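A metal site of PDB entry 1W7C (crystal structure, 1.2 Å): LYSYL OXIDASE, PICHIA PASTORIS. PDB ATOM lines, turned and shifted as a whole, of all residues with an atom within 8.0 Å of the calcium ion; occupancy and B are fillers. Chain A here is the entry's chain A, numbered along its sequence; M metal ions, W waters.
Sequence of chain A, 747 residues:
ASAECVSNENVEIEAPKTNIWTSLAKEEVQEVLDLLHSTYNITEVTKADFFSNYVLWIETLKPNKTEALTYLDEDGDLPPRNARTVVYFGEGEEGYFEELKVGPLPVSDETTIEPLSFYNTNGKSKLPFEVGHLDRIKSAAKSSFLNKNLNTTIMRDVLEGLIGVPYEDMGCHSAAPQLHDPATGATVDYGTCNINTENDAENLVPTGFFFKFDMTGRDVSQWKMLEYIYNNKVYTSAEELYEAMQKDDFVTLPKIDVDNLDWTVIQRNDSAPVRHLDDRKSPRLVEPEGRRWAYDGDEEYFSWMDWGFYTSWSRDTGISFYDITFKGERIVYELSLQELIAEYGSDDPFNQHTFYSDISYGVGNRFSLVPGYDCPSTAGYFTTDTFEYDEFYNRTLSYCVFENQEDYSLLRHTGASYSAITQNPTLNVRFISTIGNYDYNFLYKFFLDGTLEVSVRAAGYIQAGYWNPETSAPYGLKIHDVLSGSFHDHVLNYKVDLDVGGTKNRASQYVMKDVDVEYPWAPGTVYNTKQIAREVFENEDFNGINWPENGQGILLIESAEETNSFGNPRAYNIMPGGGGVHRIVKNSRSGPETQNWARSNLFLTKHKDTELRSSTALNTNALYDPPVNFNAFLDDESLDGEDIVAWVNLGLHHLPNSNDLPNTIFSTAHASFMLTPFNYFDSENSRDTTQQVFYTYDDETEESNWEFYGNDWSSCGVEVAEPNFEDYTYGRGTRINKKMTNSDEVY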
ATOM      1  N   LYS A  65      -0.064 -23.853 -21.969  1.00  0.00           N
ATOM      2  CA  LYS A  65      -1.346 -23.293 -21.612  1.00  0.00           C
ATOM      3  C   LYS A  65      -2.126 -24.154 -20.626  1.00  0.00           C
ATOM      4  O   LYS A  65      -2.671 -23.619 -19.679  1.00  0.00           O
ATOM      5  CB  LYS A  65      -2.182 -22.992 -22.860  1.00  0.00           C
ATOM      6  CG  LYS A  65      -3.546 -22.385 -22.533  1.00  0.00           C
ATOM      7  CD  LYS A  65      -4.263 -21.907 -23.794  1.00  0.00           C
ATOM      8  CE  LYS A  65      -5.589 -21.291 -23.430  1.00  0.00           C
ATOM      9  NZ  LYS A  65      -6.268 -20.796 -24.661  1.00  0.00           N
ATOM     10  N   ILE A 331     -11.393 -13.387 -20.669  1.00  0.00           N
ATOM     11  CA  ILE A 331     -11.759 -13.305 -22.080  1.00  0.00           C
ATOM     12  C   ILE A 331     -10.612 -13.609 -23.037  1.00  0.00           C
ATOM     13  O   ILE A 331     -10.863 -14.073 -24.135  1.00  0.00           O
ATOM     14  CB  ILE A 331     -12.423 -11.970 -22.431  1.00  0.00           C
ATOM     15  CG1 ILE A 331     -11.518 -10.778 -22.200  1.00  0.00           C
ATOM     16  CG2 ILE A 331     -13.774 -11.811 -21.715  1.00  0.00           C
ATOM     17  CD1 ILE A 331     -11.930  -9.543 -22.939  1.00  0.00           C
ATOM     18  N   VAL A 332      -9.369 -13.347 -22.614  1.00  0.00           N
ATOM     19  CA  VAL A 332      -8.206 -13.593 -23.491  1.00  0.00           C
ATOM     20  C   VAL A 332      -7.085 -14.195 -22.633  1.00  0.00           C
ATOM     21  O   VAL A 332      -6.648 -13.587 -21.661  1.00  0.00           O
ATOM     22  CB  VAL A 332      -7.695 -12.270 -24.142  1.00  0.00           C
ATOM     23  CG1 VAL A 332      -6.381 -12.520 -24.910  1.00  0.00           C
ATOM     24  CG2 VAL A 332      -8.731 -11.626 -25.022  1.00  0.00           C
ATOM     25  N   TYR A 333      -6.636 -15.386 -23.023  1.00  0.00           N
ATOM     26  CA  TYR A 333      -5.525 -16.019 -22.339  1.00  0.00           C
ATOM     27  C   TYR A 333      -4.205 -15.306 -22.610  1.00  0.00           C
ATOM     28  O   TYR A 333      -3.450 -15.012 -21.690  1.00  0.00           O
ATOM     29  CB  TYR A 333      -5.432 -17.523 -22.673  1.00  0.00           C
ATOM     30  CG  TYR A 333      -4.148 -18.108 -22.070  1.00  0.00           C
ATOM     31  CD1 TYR A 333      -4.056 -18.316 -20.714  1.00  0.00           C
ATOM     32  CD2 TYR A 333      -3.045 -18.401 -22.865  1.00  0.00           C
ATOM     33  CE1 TYR A 333      -2.861 -18.760 -20.143  1.00  0.00           C
ATOM     34  CE2 TYR A 333      -1.857 -18.854 -22.323  1.00  0.00           C
ATOM     35  CZ  TYR A 333      -1.781 -19.038 -20.944  1.00  0.00           C
ATOM     36  OH  TYR A 333      -0.612 -19.445 -20.382  1.00  0.00           O
ATOM     37  N   GLU A 334      -3.966 -15.011 -23.895  1.00  0.00           N
ATOM     38  CA  GLU A 334      -2.742 -14.363 -24.360  1.00  0.00           C
ATOM     39  C   GLU A 334      -3.082 -13.389 -25.464  1.00  0.00           C
ATOM     40  O   GLU A 334      -3.792 -13.773 -26.390  1.00  0.00           O
ATOM     41  CB  GLU A 334      -1.787 -15.430 -24.927  1.00  0.00           C
ATOM     42  CG  GLU A 334      -0.495 -14.845 -25.511  1.00  0.00           C
ATOM     43  CD  GLU A 334       0.485 -15.846 -26.079  1.00  0.00           C
ATOM     44  OE1 GLU A 334       1.524 -15.367 -26.587  1.00  0.00           O
ATOM     45  OE2 GLU A 334       0.241 -17.078 -26.029  1.00  0.00           O
ATOM     46  N   VAL A 496      -4.107 -13.436 -30.819  1.00  0.00           N
ATOM     47  CA  VAL A 496      -5.253 -13.054 -30.004  1.00  0.00           C
ATOM     48  C   VAL A 496      -5.936 -14.346 -29.576  1.00  0.00           C
ATOM     49  O   VAL A 496      -6.815 -14.886 -30.271  1.00  0.00           O
ATOM     50  CB  VAL A 496      -6.229 -12.142 -30.812  1.00  0.00           C
ATOM     51  CG1 VAL A 496      -7.368 -11.663 -29.943  1.00  0.00           C
ATOM     52  CG2 VAL A 496      -5.516 -10.935 -31.434  1.00  0.00           C
ATOM     53  N   ASP A 497      -5.525 -14.865 -28.436  1.00  0.00           N
ATOM     54  CA  ASP A 497      -6.049 -16.124 -27.939  1.00  0.00           C
ATOM     55  C   ASP A 497      -7.241 -15.837 -27.048  1.00  0.00           C
ATOM     56  O   ASP A 497      -7.219 -15.935 -25.817  1.00  0.00           O
ATOM     57  CB  ASP A 497      -4.955 -16.925 -27.245  1.00  0.00           C
ATOM     58  CG  ASP A 497      -5.414 -18.245 -26.755  1.00  0.00           C
ATOM     59  OD1 ASP A 497      -6.545 -18.697 -27.153  1.00  0.00           O
ATOM     60  OD2 ASP A 497      -4.664 -18.915 -25.998  1.00  0.00           O
ATOM     61  N   LEU A 498      -8.348 -15.509 -27.716  1.00  0.00           N
ATOM     62  CA  LEU A 498      -9.649 -15.333 -27.084  1.00  0.00           C
ATOM     63  C   LEU A 498     -10.071 -16.693 -26.536  1.00  0.00           C
ATOM     64  O   LEU A 498      -9.962 -17.699 -27.249  1.00  0.00           O
ATOM     65  CB  LEU A 498     -10.695 -14.833 -28.121  1.00  0.00           C
ATOM     66  CG  LEU A 498     -10.692 -13.312 -28.314  1.00  0.00           C
ATOM     67  CD1 LEU A 498     -11.162 -12.970 -29.739  1.00  0.00           C
ATOM     68  CD2 LEU A 498     -11.559 -12.633 -27.294  1.00  0.00           C
ATOM     69  N   ASP A 499     -10.642 -16.696 -25.341  1.00  0.00           N
ATOM     70  CA  ASP A 499     -11.230 -17.881 -24.710  1.00  0.00           C
ATOM     71  C   ASP A 499     -12.589 -17.384 -24.182  1.00  0.00           C
ATOM     72  O   ASP A 499     -12.711 -16.962 -23.017  1.00  0.00           O
ATOM     73  CB  ASP A 499     -10.387 -18.384 -23.531  1.00  0.00           C
ATOM     74  CG  ASP A 499      -9.159 -19.170 -23.916  1.00  0.00           C
ATOM     75  OD1 ASP A 499      -8.941 -19.531 -25.095  1.00  0.00           O
ATOM     76  OD2 ASP A 499      -8.338 -19.442 -22.971  1.00  0.00           O
ATOM     77  N   VAL A 500     -13.573 -17.318 -25.049  1.00  0.00           N
ATOM     78  CA  VAL A 500     -14.848 -16.721 -24.695  1.00  0.00           C
ATOM     79  C   VAL A 500     -15.741 -17.724 -23.995  1.00  0.00           C
ATOM     80  O   VAL A 500     -16.137 -18.723 -24.575  1.00  0.00           O
ATOM     81  CB  VAL A 500     -15.570 -16.157 -25.953  1.00  0.00           C
ATOM     82  CG1 VAL A 500     -16.827 -15.456 -25.540  1.00  0.00           C
ATOM     83  CG2 VAL A 500     -14.648 -15.213 -26.679  1.00  0.00           C
ATOM     84  N   GLY A 502     -14.878 -19.794 -21.628  1.00  0.00           N
ATOM     85  CA  GLY A 502     -14.025 -20.964 -21.593  1.00  0.00           C
ATOM     86  C   GLY A 502     -13.160 -21.143 -22.817  1.00  0.00           C
ATOM     87  O   GLY A 502     -13.220 -20.332 -23.749  1.00  0.00           O
ATOM     88  N   THR A 503     -12.308 -22.160 -22.827  1.00  0.00           N
ATOM     89  CA  THR A 503     -11.487 -22.415 -24.002  1.00  0.00           C
ATOM     90  C   THR A 503     -12.235 -22.942 -25.205  1.00  0.00           C
ATOM     91  O   THR A 503     -11.860 -22.668 -26.365  1.00  0.00           O
ATOM     92  CB  THR A 503     -10.331 -23.393 -23.691  1.00  0.00           C
ATOM     93  OG1 THR A 503     -10.852 -24.640 -23.179  1.00  0.00           O
ATOM     94  CG2 THR A 503      -9.346 -22.831 -22.685  1.00  0.00           C
ATOM     95  N   LYS A 504     -13.247 -23.770 -24.976  1.00  0.00           N
ATOM     96  CA  LYS A 504     -13.912 -24.469 -26.061  1.00  0.00           C
ATOM     97  C   LYS A 504     -14.845 -23.490 -26.765  1.00  0.00           C
ATOM     98  O   LYS A 504     -15.864 -23.070 -26.176  1.00  0.00           O
ATOM     99  CB  LYS A 504     -14.694 -25.712 -25.562  1.00  0.00           C
ATOM    100  CG  LYS A 504     -15.240 -26.550 -26.660  1.00  0.00           C
ATOM    101  CD  LYS A 504     -16.126 -27.739 -26.189  1.00  0.00           C
ATOM    102  CE  LYS A 504     -16.640 -28.589 -27.372  1.00  0.00           C
ATOM    103  NZ  LYS A 504     -17.417 -29.759 -26.875  1.00  0.00           N
ATOM    104  N   ASN A 505     -14.495 -23.138 -28.001  1.00  0.00           N
ATOM    105  CA  ASN A 505     -15.140 -22.069 -28.725  1.00  0.00           C
ATOM    106  C   ASN A 505     -15.485 -22.508 -30.157  1.00  0.00           C
ATOM    107  O   ASN A 505     -15.157 -23.612 -30.597  1.00  0.00           O
ATOM    108  CB  ASN A 505     -14.221 -20.819 -28.799  1.00  0.00           C
ATOM    109  CG  ASN A 505     -14.005 -20.075 -27.469  1.00  0.00           C
ATOM    110  OD1 ASN A 505     -13.211 -19.131 -27.463  1.00  0.00           O
ATOM    111  ND2 ASN A 505     -14.713 -20.427 -26.385  1.00  0.00           N
ATOM    112  N   ILE A 557     -15.935 -14.848 -32.186  1.00  0.00           N
ATOM    113  CA  ILE A 557     -15.534 -16.000 -31.428  1.00  0.00           C
ATOM    114  C   ILE A 557     -16.596 -16.241 -30.364  1.00  0.00           C
ATOM    115  O   ILE A 557     -16.820 -15.403 -29.497  1.00  0.00           O
ATOM    116  CB  ILE A 557     -14.152 -15.831 -30.806  1.00  0.00           C
ATOM    117  CG1 ILE A 557     -13.090 -15.474 -31.878  1.00  0.00           C
ATOM    118  CG2 ILE A 557     -13.773 -17.073 -29.993  1.00  0.00           C
ATOM    119  CD1 ILE A 557     -12.882 -16.454 -32.976  1.00  0.00           C
ATOM    120  N   THR A 605      -6.806 -20.612 -35.980  1.00  0.00           N
ATOM    121  CA  THR A 605      -6.222 -21.934 -35.821  1.00  0.00           C
ATOM    122  C   THR A 605      -6.607 -22.560 -34.509  1.00  0.00           C
ATOM    123  O   THR A 605      -7.048 -21.894 -33.564  1.00  0.00           O
ATOM    124  CB  THR A 605      -4.695 -21.887 -35.899  1.00  0.00           C
ATOM    125  OG1 THR A 605      -4.186 -21.157 -34.767  1.00  0.00           O
ATOM    126  CG2 THR A 605      -4.197 -21.202 -37.200  1.00  0.00           C
ATOM    127  N   LYS A 606      -6.394 -23.874 -34.430  1.00  0.00           N
ATOM    128  CA  LYS A 606      -6.518 -24.600 -33.174  1.00  0.00           C
ATOM    129  C   LYS A 606      -5.311 -24.309 -32.306  1.00  0.00           C
ATOM    130  O   LYS A 606      -4.176 -24.485 -32.731  1.00  0.00           O
ATOM    131  CB  LYS A 606      -6.694 -26.103 -33.467  1.00  0.00           C
ATOM    132  CG  LYS A 606      -6.658 -27.007 -32.279  1.00  0.00           C
ATOM    133  CD  LYS A 606      -6.711 -28.491 -32.734  1.00  0.00           C
ATOM    134  CE  LYS A 606      -6.582 -29.452 -31.647  1.00  0.00           C
ATOM    135  NZ  LYS A 606      -6.803 -30.784 -32.201  1.00  0.00           N
ATOM    136  N   HIS A 607      -5.548 -23.931 -31.075  1.00  0.00           N
ATOM    137  CA  HIS A 607      -4.472 -23.618 -30.146  1.00  0.00           C
ATOM    138  C   HIS A 607      -3.553 -24.805 -29.975  1.00  0.00           C
ATOM    139  O   HIS A 607      -4.023 -25.921 -29.764  1.00  0.00           O
ATOM    140  CB  HIS A 607      -4.992 -23.259 -28.771  1.00  0.00           C
ATOM    141  CG  HIS A 607      -3.892 -22.900 -27.817  1.00  0.00           C
ATOM    142  ND1 HIS A 607      -3.206 -23.857 -27.105  1.00  0.00           N
ATOM    143  CD2 HIS A 607      -3.276 -21.728 -27.589  1.00  0.00           C
ATOM    144  CE1 HIS A 607      -2.223 -23.259 -26.433  1.00  0.00           C
ATOM    145  NE2 HIS A 607      -2.271 -21.959 -26.684  1.00  0.00           N
ATOM    146  N   GLU A 642     -13.507 -26.032 -30.148  1.00  0.00           N
ATOM    147  CA  GLU A 642     -12.093 -26.193 -29.945  1.00  0.00           C
ATOM    148  C   GLU A 642     -11.537 -24.913 -29.347  1.00  0.00           C
ATOM    149  O   GLU A 642     -12.183 -23.876 -29.417  1.00  0.00           O
ATOM    150  CB  GLU A 642     -11.386 -26.522 -31.267  1.00  0.00           C
ATOM    151  CG  GLU A 642     -11.787 -27.861 -31.880  1.00  0.00           C
ATOM    152  CD  GLU A 642     -11.411 -29.101 -31.080  1.00  0.00           C
ATOM    153  OE1 GLU A 642     -10.502 -29.064 -30.234  1.00  0.00           O
ATOM    154  OE2 GLU A 642     -12.049 -30.135 -31.314  1.00  0.00           O
ATOM    155  N   ASP A 643     -10.334 -24.984 -28.805  1.00  0.00           N
ATOM    156  CA  ASP A 643      -9.618 -23.777 -28.374  1.00  0.00           C
ATOM    157  C   ASP A 643      -9.041 -23.118 -29.612  1.00  0.00           C
ATOM    158  O   ASP A 643      -8.205 -23.707 -30.318  1.00  0.00           O
ATOM    159  CB  ASP A 643      -8.524 -24.178 -27.405  1.00  0.00           C
ATOM    160  CG  ASP A 643      -7.832 -23.014 -26.789  1.00  0.00           C
ATOM    161  OD1 ASP A 643      -8.061 -21.868 -27.229  1.00  0.00           O
ATOM    162  OD2 ASP A 643      -7.050 -23.185 -25.807  1.00  0.00           O
ATOM    163  N   ILE A 644      -9.562 -21.937 -29.932  1.00  0.00           N
ATOM    164  CA  ILE A 644      -9.232 -21.208 -31.145  1.00  0.00           C
ATOM    165  C   ILE A 644      -8.307 -20.059 -30.763  1.00  0.00           C
ATOM    166  O   ILE A 644      -8.414 -19.438 -29.692  1.00  0.00           O
ATOM    167  CB  ILE A 644     -10.535 -20.671 -31.796  1.00  0.00           C
ATOM    168  CG1 ILE A 644     -11.441 -21.838 -32.193  1.00  0.00           C
ATOM    169  CG2 ILE A 644     -10.227 -19.782 -33.018  1.00  0.00           C
ATOM    170  CD1 ILE A 644     -12.807 -21.450 -32.678  1.00  0.00           C
ATOM    171  N   VAL A 645      -7.377 -19.791 -31.684  1.00  0.00           N
ATOM    172  CA  VAL A 645      -6.538 -18.601 -31.637  1.00  0.00           C
ATOM    173  C   VAL A 645      -6.792 -17.816 -32.946  1.00  0.00           C
ATOM    174  O   VAL A 645      -6.847 -18.414 -34.038  1.00  0.00           O
ATOM    175  CB  VAL A 645      -5.025 -18.980 -31.596  1.00  0.00           C
ATOM    176  CG1 VAL A 645      -4.136 -17.760 -31.631  1.00  0.00           C
ATOM    177  CG2 VAL A 645      -4.734 -19.870 -30.420  1.00  0.00           C
ATOM    178  N   ALA A 646      -6.992 -16.500 -32.805  1.00  0.00           N
ATOM    179  CA  ALA A 646      -7.052 -15.623 -33.970  1.00  0.00           C
ATOM    180  C   ALA A 646      -5.717 -14.908 -34.096  1.00  0.00           C
ATOM    181  O   ALA A 646      -5.231 -14.325 -33.179  1.00  0.00           O
ATOM    182  CB  ALA A 646      -8.184 -14.619 -33.845  1.00  0.00           C
HETATM  183 CA    CA M   1      -8.614 -19.619 -27.342  1.00  0.00          CA
HETATM  184  O   HOH W   1     -10.853 -20.519 -27.624  1.00  0.00           O
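The backbone carbonyl oxygen of Ile 331 lies within hydrogen-bond range of the backbone NH of Asp 499 (2.9 Å).
The backbone carbonyl oxygen (O) of Asp 497 lies within hydrogen-bond range of the backbone NH (N) of Tyr 333 (2.9 Å).
The backbone carbonyl oxygen (O) of Asp 643 is in hydrogen-bond range of the backbone NH (N) of His 607.
N of Asp 497 is in hydrogen-bond range of O of Glu 334 (2.9 Å).
NZ of Lys 65 is in salt-bridge range of OD2 of Asp 499, 3.0 Å away.
The side-chain carboxylate of Asp 643 is in salt-bridge range of the side-chain amino group of Lys 65.
The side-chain carboxylate (OD2) of Asp 497 lies within salt-bridge range of the side-chain amino group (NZ) of Lys 65 (2.8 Å).
The calcium ion is bound by the side-chain carboxylate of Asp 499 (2.3 Å), the side-chain carboxylate of Asp 497 (2.3 Å), the side-chain carboxylate of Asp 643 (2.3 Å), the backbone carbonyl oxygen of Leu 498 (2.3 Å), the backbone carbonyl oxygen of Ile 644 (2.4 Å) and water W1 (2.4 Å).
Residues that only touch the calcium ion: Lys 65 (3.8 Å).
Within 4 Å of the calcium ion: Lys 65, Asp 497, Leu 498, Asp 499, Asp 643 and Ile 644.
Water W1 lies within hydrogen-bond range of the backbone carbonyl oxygen of Thr 503 (2.7 Å), the side-chain amide oxygen of Asn 505 (2.7 Å) and the backbone NH of Ile 644 (3.0 Å).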
